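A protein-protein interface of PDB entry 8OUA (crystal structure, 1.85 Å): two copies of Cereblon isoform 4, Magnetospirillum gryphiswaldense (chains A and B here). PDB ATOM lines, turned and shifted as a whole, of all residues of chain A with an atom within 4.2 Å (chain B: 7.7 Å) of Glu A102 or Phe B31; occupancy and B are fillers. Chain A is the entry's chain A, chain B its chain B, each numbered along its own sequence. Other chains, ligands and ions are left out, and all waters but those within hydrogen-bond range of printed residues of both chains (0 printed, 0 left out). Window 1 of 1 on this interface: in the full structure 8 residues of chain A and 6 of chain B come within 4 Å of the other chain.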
ATOM      1  N   SER A   2      -6.749 -12.753  -6.897  1.00  0.00           N
ATOM      2  CA  SER A   2      -6.503 -13.653  -5.756  1.00  0.00           C
ATOM      3  C   SER A   2      -5.655 -13.031  -4.650  1.00  0.00           C
ATOM      4  O   SER A   2      -5.974 -13.384  -3.533  1.00  0.00           O
ATOM      5  CB  SER A   2      -5.992 -15.032  -6.100  1.00  0.00           C
ATOM      6  OG  SER A   2      -4.756 -14.976  -6.740  1.00  0.00           O
ATOM      7  N   ILE A   3      -4.648 -12.166  -4.874  1.00  0.00           N
ATOM      8  CA  ILE A   3      -3.861 -11.557  -3.774  1.00  0.00           C
ATOM      9  C   ILE A   3      -4.212 -10.063  -3.657  1.00  0.00           C
ATOM     10  O   ILE A   3      -4.501  -9.394  -4.657  1.00  0.00           O
ATOM     11  CB  ILE A   3      -2.376 -11.733  -4.083  1.00  0.00           C
ATOM     12  CG1 ILE A   3      -2.018 -13.221  -3.949  1.00  0.00           C
ATOM     13  CG2 ILE A   3      -1.491 -10.894  -3.230  1.00  0.00           C
ATOM     14  CD1 ILE A   3      -0.539 -13.477  -3.835  1.00  0.00           C
ATOM     15  N   PHE A   4      -4.262  -9.589  -2.449  1.00  0.00           N
ATOM     16  CA  PHE A   4      -4.399  -8.166  -2.156  1.00  0.00           C
ATOM     17  C   PHE A   4      -3.064  -7.550  -1.735  1.00  0.00           C
ATOM     18  O   PHE A   4      -2.466  -8.007  -0.798  1.00  0.00           O
ATOM     19  CB  PHE A   4      -5.450  -7.955  -1.123  1.00  0.00           C
ATOM     20  CG  PHE A   4      -6.844  -8.269  -1.548  1.00  0.00           C
ATOM     21  CD1 PHE A   4      -7.533  -7.435  -2.396  1.00  0.00           C
ATOM     22  CD2 PHE A   4      -7.440  -9.483  -1.167  1.00  0.00           C
ATOM     23  CE1 PHE A   4      -8.843  -7.768  -2.784  1.00  0.00           C
ATOM     24  CE2 PHE A   4      -8.762  -9.762  -1.499  1.00  0.00           C
ATOM     25  CZ  PHE A   4      -9.413  -8.950  -2.379  1.00  0.00           C
ATOM     26  N   ARG A   5      -2.711  -6.426  -2.399  1.00  0.00           N
ATOM     27  CA  ARG A   5      -1.535  -5.636  -2.098  1.00  0.00           C
ATOM     28  C   ARG A   5      -1.958  -4.234  -1.649  1.00  0.00           C
ATOM     29  O   ARG A   5      -3.040  -3.845  -1.940  1.00  0.00           O
ATOM     30  CB  ARG A   5      -0.627  -5.605  -3.320  1.00  0.00           C
ATOM     31  CG  ARG A   5       0.074  -6.942  -3.616  1.00  0.00           C
ATOM     32  CD  ARG A   5       0.989  -6.876  -4.832  1.00  0.00           C
ATOM     33  NE  ARG A   5       1.608  -8.189  -5.052  1.00  0.00           N
ATOM     34  CZ  ARG A   5       2.541  -8.744  -4.273  1.00  0.00           C
ATOM     35  NH1 ARG A   5       3.113  -8.066  -3.297  1.00  0.00           N
ATOM     36  NH2 ARG A   5       2.880  -9.986  -4.459  1.00  0.00           N
ATOM     37  N   ARG A  16      -7.890 -13.309  -1.359  1.00  0.00           N
ATOM     38  CA  ARG A  16      -9.328 -13.461  -1.471  1.00  0.00           C
ATOM     39  C   ARG A  16      -9.789 -14.718  -0.659  1.00  0.00           C
ATOM     40  O   ARG A  16     -10.833 -14.704  -0.056  1.00  0.00           O
ATOM     41  CB  ARG A  16      -9.712 -13.550  -2.960  1.00  0.00           C
ATOM     42  CG  ARG A  16     -11.216 -13.629  -3.208  1.00  0.00           C
ATOM     43  CD  ARG A  16     -11.660 -13.213  -4.613  1.00  0.00           C
ATOM     44  NE  ARG A  16     -11.732 -11.764  -4.902  1.00  0.00           N
ATOM     45  CZ  ARG A  16     -12.746 -10.954  -4.611  1.00  0.00           C
ATOM     46  NH1 ARG A  16     -13.939 -11.412  -4.268  1.00  0.00           N
ATOM     47  NH2 ARG A  16     -12.582  -9.651  -4.676  1.00  0.00           N
ATOM     48  N   ALA A 101      -5.113  -3.290  -3.672  1.00  0.00           N
ATOM     49  CA  ALA A 101      -5.133  -3.636  -5.088  1.00  0.00           C
ATOM     50  C   ALA A 101      -5.145  -5.142  -5.248  1.00  0.00           C
ATOM     51  O   ALA A 101      -4.295  -5.821  -4.665  1.00  0.00           O
ATOM     52  CB  ALA A 101      -3.992  -2.992  -5.803  1.00  0.00           C
ATOM     53  N   GLU A 102      -6.095  -5.647  -6.069  1.00  0.00           N
ATOM     54  CA  GLU A 102      -6.256  -7.088  -6.243  1.00  0.00           C
ATOM     55  C   GLU A 102      -5.557  -7.594  -7.481  1.00  0.00           C
ATOM     56  O   GLU A 102      -5.624  -6.978  -8.556  1.00  0.00           O
ATOM     57  CB  GLU A 102      -7.741  -7.413  -6.269  1.00  0.00           C
ATOM     58  CG  GLU A 102      -8.026  -8.945  -6.354  1.00  0.00           C
ATOM     59  CD  GLU A 102      -9.498  -9.373  -6.281  1.00  0.00           C
ATOM     60  OE1 GLU A 102     -10.393  -8.450  -6.206  1.00  0.00           O
ATOM     61  OE2 GLU A 102      -9.746 -10.599  -6.153  1.00  0.00           O
ATOM     62  N   GLY A 103      -4.909  -8.740  -7.388  1.00  0.00           N
ATOM     63  CA  GLY A 103      -4.277  -9.211  -8.616  1.00  0.00           C
ATOM     64  C   GLY A 103      -3.710 -10.608  -8.509  1.00  0.00           C
ATOM     65  O   GLY A 103      -3.921 -11.353  -7.505  1.00  0.00           O
ATOM     66  N   PRO A 104      -3.009 -11.046  -9.590  1.00  0.00           N
ATOM     67  CA  PRO A 104      -2.458 -12.414  -9.634  1.00  0.00           C
ATOM     68  C   PRO A 104      -1.452 -12.857  -8.567  1.00  0.00           C
ATOM     69  O   PRO A 104      -0.625 -12.083  -8.084  1.00  0.00           O
ATOM     70  CB  PRO A 104      -1.770 -12.535 -11.021  1.00  0.00           C
ATOM     71  CG  PRO A 104      -1.590 -11.077 -11.460  1.00  0.00           C
ATOM     72  CD  PRO A 104      -2.742 -10.320 -10.830  1.00  0.00           C
ATOM     73  N   HIS B  28     -12.903  -1.548  -9.326  1.00  0.00           N
ATOM     74  CA  HIS B  28     -11.914  -2.494  -8.864  1.00  0.00           C
ATOM     75  C   HIS B  28     -10.532  -1.832  -8.963  1.00  0.00           C
ATOM     76  O   HIS B  28     -10.111  -1.486 -10.072  1.00  0.00           O
ATOM     77  CB  HIS B  28     -11.996  -3.739  -9.741  1.00  0.00           C
ATOM     78  CG  HIS B  28     -13.318  -4.435  -9.618  1.00  0.00           C
ATOM     79  ND1 HIS B  28     -13.481  -5.635  -8.963  1.00  0.00           N
ATOM     80  CD2 HIS B  28     -14.538  -4.051 -10.045  1.00  0.00           C
ATOM     81  CE1 HIS B  28     -14.787  -5.918  -8.917  1.00  0.00           C
ATOM     82  NE2 HIS B  28     -15.451  -4.993  -9.548  1.00  0.00           N
ATOM     83  N   VAL B  29      -9.773  -1.851  -7.874  1.00  0.00           N
ATOM     84  CA  VAL B  29      -8.342  -1.529  -7.942  1.00  0.00           C
ATOM     85  C   VAL B  29      -7.562  -2.841  -8.130  1.00  0.00           C
ATOM     86  O   VAL B  29      -7.737  -3.778  -7.340  1.00  0.00           O
ATOM     87  CB  VAL B  29      -7.889  -0.725  -6.723  1.00  0.00           C
ATOM     88  CG1 VAL B  29      -6.411  -0.334  -6.776  1.00  0.00           C
ATOM     89  CG2 VAL B  29      -8.745   0.549  -6.514  1.00  0.00           C
ATOM     90  N   VAL B  30      -6.776  -2.923  -9.176  1.00  0.00           N
ATOM     91  CA  VAL B  30      -6.158  -4.140  -9.650  1.00  0.00           C
ATOM     92  C   VAL B  30      -4.678  -3.890  -9.940  1.00  0.00           C
ATOM     93  O   VAL B  30      -4.275  -2.713 -10.167  1.00  0.00           O
ATOM     94  CB  VAL B  30      -6.918  -4.729 -10.830  1.00  0.00           C
ATOM     95  CG1 VAL B  30      -8.340  -5.241 -10.469  1.00  0.00           C
ATOM     96  CG2 VAL B  30      -6.949  -3.742 -11.986  1.00  0.00           C
ATOM     97  N   PHE B  31      -3.876  -5.001  -9.991  1.00  0.00           N
ATOM     98  CA  PHE B  31      -2.479  -4.943 -10.422  1.00  0.00           C
ATOM     99  C   PHE B  31      -2.177  -6.102 -11.367  1.00  0.00           C
ATOM    100  O   PHE B  31      -2.780  -7.144 -11.269  1.00  0.00           O
ATOM    101  CB  PHE B  31      -1.456  -4.911  -9.271  1.00  0.00           C
ATOM    102  CG  PHE B  31      -1.390  -6.175  -8.430  1.00  0.00           C
ATOM    103  CD1 PHE B  31      -0.647  -7.278  -8.855  1.00  0.00           C
ATOM    104  CD2 PHE B  31      -2.162  -6.322  -7.292  1.00  0.00           C
ATOM    105  CE1 PHE B  31      -0.629  -8.443  -8.111  1.00  0.00           C
ATOM    106  CE2 PHE B  31      -2.181  -7.518  -6.578  1.00  0.00           C
ATOM    107  CZ  PHE B  31      -1.359  -8.529  -6.949  1.00  0.00           C
ATOM    108  N   ASN B  32      -1.432  -5.790 -12.433  1.00  0.00           N
ATOM    109  CA  ASN B  32      -1.080  -6.770 -13.472  1.00  0.00           C
ATOM    110  C   ASN B  32       0.193  -7.488 -13.035  1.00  0.00           C
ATOM    111  O   ASN B  32       0.805  -7.167 -12.018  1.00  0.00           O
ATOM    112  CB  ASN B  32      -1.100  -6.037 -14.830  1.00  0.00           C
ATOM    113  CG  ASN B  32       0.133  -5.207 -15.146  1.00  0.00           C
ATOM    114  OD1 ASN B  32       1.086  -5.187 -14.380  1.00  0.00           O
ATOM    115  ND2 ASN B  32       0.113  -4.538 -16.309  1.00  0.00           N
ATOM    116  N   PRO B  33       0.685  -8.505 -13.788  1.00  0.00           N
ATOM    117  CA  PRO B  33       1.911  -9.188 -13.402  1.00  0.00           C
ATOM    118  C   PRO B  33       3.194  -8.362 -13.497  1.00  0.00           C
ATOM    119  O   PRO B  33       4.168  -8.810 -12.870  1.00  0.00           O
ATOM    120  CB  PRO B  33       2.055 -10.384 -14.357  1.00  0.00           C
ATOM    121  CG  PRO B  33       0.594 -10.531 -14.903  1.00  0.00           C
ATOM    122  CD  PRO B  33       0.027  -9.122 -14.941  1.00  0.00           C
ATOM    123  N   ALA B  34       3.197  -7.250 -14.198  1.00  0.00           N
ATOM    124  CA  ALA B  34       4.327  -6.346 -14.164  1.00  0.00           C
ATOM    125  C   ALA B  34       4.230  -5.351 -12.982  1.00  0.00           C
ATOM    126  O   ALA B  34       5.101  -4.486 -12.792  1.00  0.00           O
ATOM    127  CB  ALA B  34       4.408  -5.621 -15.526  1.00  0.00           C
ATOM    128  N   GLY B  35       3.250  -5.531 -12.105  1.00  0.00           N
ATOM    129  CA  GLY B  35       3.020  -4.723 -10.922  1.00  0.00           C
ATOM    130  C   GLY B  35       2.436  -3.362 -11.202  1.00  0.00           C
ATOM    131  O   GLY B  35       2.482  -2.488 -10.324  1.00  0.00           O
ATOM    132  N   MET B  36       1.889  -3.134 -12.395  1.00  0.00           N
ATOM    133  CA  MET B  36       1.220  -1.847 -12.623  1.00  0.00           C
ATOM    134  C   MET B  36      -0.136  -1.909 -11.969  1.00  0.00           C
ATOM    135  O   MET B  36      -0.835  -2.910 -12.129  1.00  0.00           O
ATOM    136  CB  MET B  36       1.113  -1.546 -14.118  1.00  0.00           C
ATOM    137  CG  MET B  36       2.473  -1.463 -14.805  1.00  0.00           C
ATOM    138  SD  MET B  36       2.315  -1.645 -16.688  1.00  0.00           S
ATOM    139  CE  MET B  36       3.925  -2.330 -17.101  1.00  0.00           C
ATOM    140  N   ILE B  37      -0.526  -0.830 -11.288  1.00  0.00           N
ATOM    141  CA  ILE B  37      -1.764  -0.672 -10.572  1.00  0.00           C
ATOM    142  C   ILE B  37      -2.715   0.239 -11.358  1.00  0.00           C
ATOM    143  O   ILE B  37      -2.340   1.246 -11.891  1.00  0.00           O
ATOM    144  CB  ILE B  37      -1.549  -0.141  -9.156  1.00  0.00           C
ATOM    145  CG1 ILE B  37      -0.810  -1.193  -8.347  1.00  0.00           C
ATOM    146  CG2 ILE B  37      -2.844   0.246  -8.460  1.00  0.00           C
ATOM    147  CD1 ILE B  37      -0.384  -0.731  -6.977  1.00  0.00           C
ATOM    148  N   PHE B  38      -3.952  -0.218 -11.541  1.00  0.00           N
ATOM    149  CA  PHE B  38      -5.016   0.496 -12.269  1.00  0.00           C
ATOM    150  C   PHE B  38      -6.280   0.498 -11.436  1.00  0.00           C
ATOM    151  O   PHE B  38      -6.621  -0.468 -10.704  1.00  0.00           O
ATOM    152  CB  PHE B  38      -5.337  -0.197 -13.598  1.00  0.00           C
ATOM    153  CG  PHE B  38      -4.232  -0.471 -14.580  1.00  0.00           C
ATOM    154  CD1 PHE B  38      -3.799   0.493 -15.447  1.00  0.00           C
ATOM    155  CD2 PHE B  38      -3.483  -1.628 -14.502  1.00  0.00           C
ATOM    156  CE1 PHE B  38      -2.756   0.258 -16.333  1.00  0.00           C
ATOM    157  CE2 PHE B  38      -2.423  -1.859 -15.345  1.00  0.00           C
ATOM    158  CZ  PHE B  38      -2.061  -0.924 -16.283  1.00  0.00           C
ATOM    159  N   ARG B  39      -7.007   1.607 -11.563  1.00  0.00           N
ATOM    160  CA  ARG B  39      -8.301   1.726 -10.945  1.00  0.00           C
ATOM    161  C   ARG B  39      -9.303   1.608 -12.084  1.00  0.00           C
ATOM    162  O   ARG B  39      -9.383   2.477 -12.945  1.00  0.00           O
ATOM    163  CB  ARG B  39      -8.455   2.991 -10.083  1.00  0.00           C
ATOM    164  CG  ARG B  39      -9.832   3.185  -9.533  1.00  0.00           C
ATOM    165  CD  ARG B  39      -9.763   4.200  -8.355  1.00  0.00           C
ATOM    166  NE  ARG B  39      -9.490   5.509  -8.989  1.00  0.00           N
ATOM    167  CZ  ARG B  39     -10.423   6.448  -9.242  1.00  0.00           C
ATOM    168  NH1 ARG B  39     -11.689   6.198  -9.061  1.00  0.00           N
ATOM    169  NH2 ARG B  39     -10.077   7.566  -9.827  1.00  0.00           N
ATOM    170  N   VAL B  40     -10.053   0.506 -12.073  1.00  0.00           N
ATOM    171  CA  VAL B  40     -10.899   0.131 -13.176  1.00  0.00           C
ATOM    172  C   VAL B  40     -12.349   0.326 -12.773  1.00  0.00           C
ATOM    173  O   VAL B  40     -12.777  -0.103 -11.704  1.00  0.00           O
ATOM    174  CB  VAL B  40     -10.604  -1.347 -13.556  1.00  0.00           C
ATOM    175  CG1 VAL B  40     -11.645  -1.993 -14.391  1.00  0.00           C
ATOM    176  CG2 VAL B  40      -9.200  -1.473 -14.119  1.00  0.00           C
ATOM    177  N   PHE B  59      -4.176 -14.405 -16.400  1.00  0.00           N
ATOM    178  CA  PHE B  59      -4.111 -13.283 -15.456  1.00  0.00           C
ATOM    179  C   PHE B  59      -5.344 -12.406 -15.452  1.00  0.00           C
ATOM    180  O   PHE B  59      -5.337 -11.294 -14.883  1.00  0.00           O
ATOM    181  CB  PHE B  59      -2.927 -12.349 -15.741  1.00  0.00           C
ATOM    182  CG  PHE B  59      -1.599 -13.057 -15.719  1.00  0.00           C
ATOM    183  CD1 PHE B  59      -1.139 -13.656 -14.565  1.00  0.00           C
ATOM    184  CD2 PHE B  59      -0.843 -13.158 -16.878  1.00  0.00           C
ATOM    185  CE1 PHE B  59       0.060 -14.351 -14.569  1.00  0.00           C
ATOM    186  CE2 PHE B  59       0.370 -13.830 -16.877  1.00  0.00           C
ATOM    187  CZ  PHE B  59       0.810 -14.431 -15.729  1.00  0.00           C
ATOM    188  N   TRP B  61      -8.370 -10.462 -14.364  1.00  0.00           N
ATOM    189  CA  TRP B  61      -8.904 -10.004 -13.091  1.00  0.00           C
ATOM    190  C   TRP B  61     -10.300 -10.562 -12.789  1.00  0.00           C
ATOM    191  O   TRP B  61     -10.770 -10.506 -11.658  1.00  0.00           O
ATOM    192  CB  TRP B  61      -8.881  -8.469 -12.990  1.00  0.00           C
ATOM    193  CG  TRP B  61      -7.493  -7.948 -12.980  1.00  0.00           C
ATOM    194  CD1 TRP B  61      -6.446  -8.353 -12.194  1.00  0.00           C
ATOM    195  CD2 TRP B  61      -7.010  -6.918 -13.830  1.00  0.00           C
ATOM    196  NE1 TRP B  61      -5.348  -7.605 -12.544  1.00  0.00           N
ATOM    197  CE2 TRP B  61      -5.670  -6.726 -13.526  1.00  0.00           C
ATOM    198  CE3 TRP B  61      -7.600  -6.125 -14.835  1.00  0.00           C
ATOM    199  CZ2 TRP B  61      -4.893  -5.779 -14.184  1.00  0.00           C
ATOM    200  CZ3 TRP B  61      -6.853  -5.152 -15.426  1.00  0.00           C
ATOM    201  CH2 TRP B  61      -5.486  -5.037 -15.172  1.00  0.00           C
ATOM    202  N   PHE B  62     -11.024 -11.007 -13.782  1.00  0.00           N
ATOM    203  CA  PHE B  62     -12.398 -11.455 -13.603  1.00  0.00           C
ATOM    204  C   PHE B  62     -12.592 -12.923 -14.038  1.00  0.00           C
ATOM    205  O   PHE B  62     -12.410 -13.287 -15.207  1.00  0.00           O
ATOM    206  CB  PHE B  62     -13.320 -10.535 -14.396  1.00  0.00           C
ATOM    207  CG  PHE B  62     -13.250  -9.081 -13.987  1.00  0.00           C
ATOM    208  CD1 PHE B  62     -13.906  -8.613 -12.872  1.00  0.00           C
ATOM    209  CD2 PHE B  62     -12.494  -8.193 -14.716  1.00  0.00           C
ATOM    210  CE1 PHE B  62     -13.823  -7.277 -12.514  1.00  0.00           C
ATOM    211  CE2 PHE B  62     -12.392  -6.864 -14.335  1.00  0.00           C
ATOM    212  CZ  PHE B  62     -13.085  -6.409 -13.257  1.00  0.00           C
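No position is printed for both chains.
Arg A16 touches none of the printed residues of chain B.
Printed residues of chain B within 4 Å of Ala A101: Val B29 (3.4 Å) and Phe B31 (3.3 Å).
Of the printed residues of chain B, Glu A102 touches Val B29, Val B30, Phe B31 and Trp B61.
Of the printed residues of chain B, Gly A103 touches Phe B31.
Printed residues of chain B within 4 Å of Pro A104: Phe B31 and Phe B59.
Of the printed residues of chain A, Val B29 touches Ala A101 (3.4 Å) and Glu A102 (2.8 Å).
Of the printed residues of chain A, Val B30 touches Glu A102 (3.1 Å).
Of the printed residues of chain A, Phe B31 touches Ile A3 (3.5 Å), Arg A5 (3.5 Å), Ala A101 (3.3 Å), Glu A102 (3.0 Å), Gly A103 (3.1 Å) and Pro A104 (3.2 Å).
Of the printed residues of chain A, Trp B61 touches Glu A102 (3.98 Å).
The nearest residue of chain B that does not touch Glu A102 is His B28 (5.0 Å).
The nearest printed residue of chain A that does not touch Phe B31 is Phe A4 (4.9 Å).
The nearest printed residue of chain B that does not touch Pro A104 is Pro B33 (4.1 Å).
O of Glu A102 sits at hydrogen-bond distance from N of Phe B31 (3.0 Å).
N of Glu A102 lies within hydrogen-bond range of O of Val B29.
Among the printed residues, pairs that only touch across the chains: Ile A3 with Phe B31, Arg A5 with Phe B31, Ala A101 with Val B29, Ala A101 with Phe B31, Glu A102 with Val B30, Glu A102 with Trp B61, Gly A103 with Phe B31, Pro A104 with Phe B31 and Pro A104 with Phe B59.
Hydrophobic or aromatic side chains of chain A that line the printed part of chain B: Ala A101 and Pro A104.
Printed residues of chain B that touch a printed residue of chain A: Val B29, Val B30, Phe B31, Phe B59 and Trp B61.
Hydrophobic or aromatic side chains of chain B that line the printed part of chain A: Val B29, Val B30, Phe B31, Phe B59 and Trp B61.
Among the printed residues, 11 pairs touch across the chains.
Among the printed residues, no Asp or Glu carboxylate lies within 4 Å of a Lys or Arg side-chain nitrogen of the other chain.
The backbone carbonyl oxygen (O) of Phe B31 is in hydrogen-bond range of the indole nitrogen (NE1) of Trp B61 (2.9 Å).
The backbone NH of Ser A2 lies within hydrogen-bond range of the backbone carbonyl oxygen of Gly A103.
N of Gly A103 sits at hydrogen-bond distance from O of Ile A3 (2.8 Å).
N of Ala A101 lies within hydrogen-bond range of O of Arg A5, at 2.8 Å.
The guanidinium group (NE) of Arg A16 lies within salt-bridge range of the side-chain carboxylate (OE2) of Glu A102 (2.6 Å).
O of Val B30 is in hydrogen-bond range of N of Phe B38.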
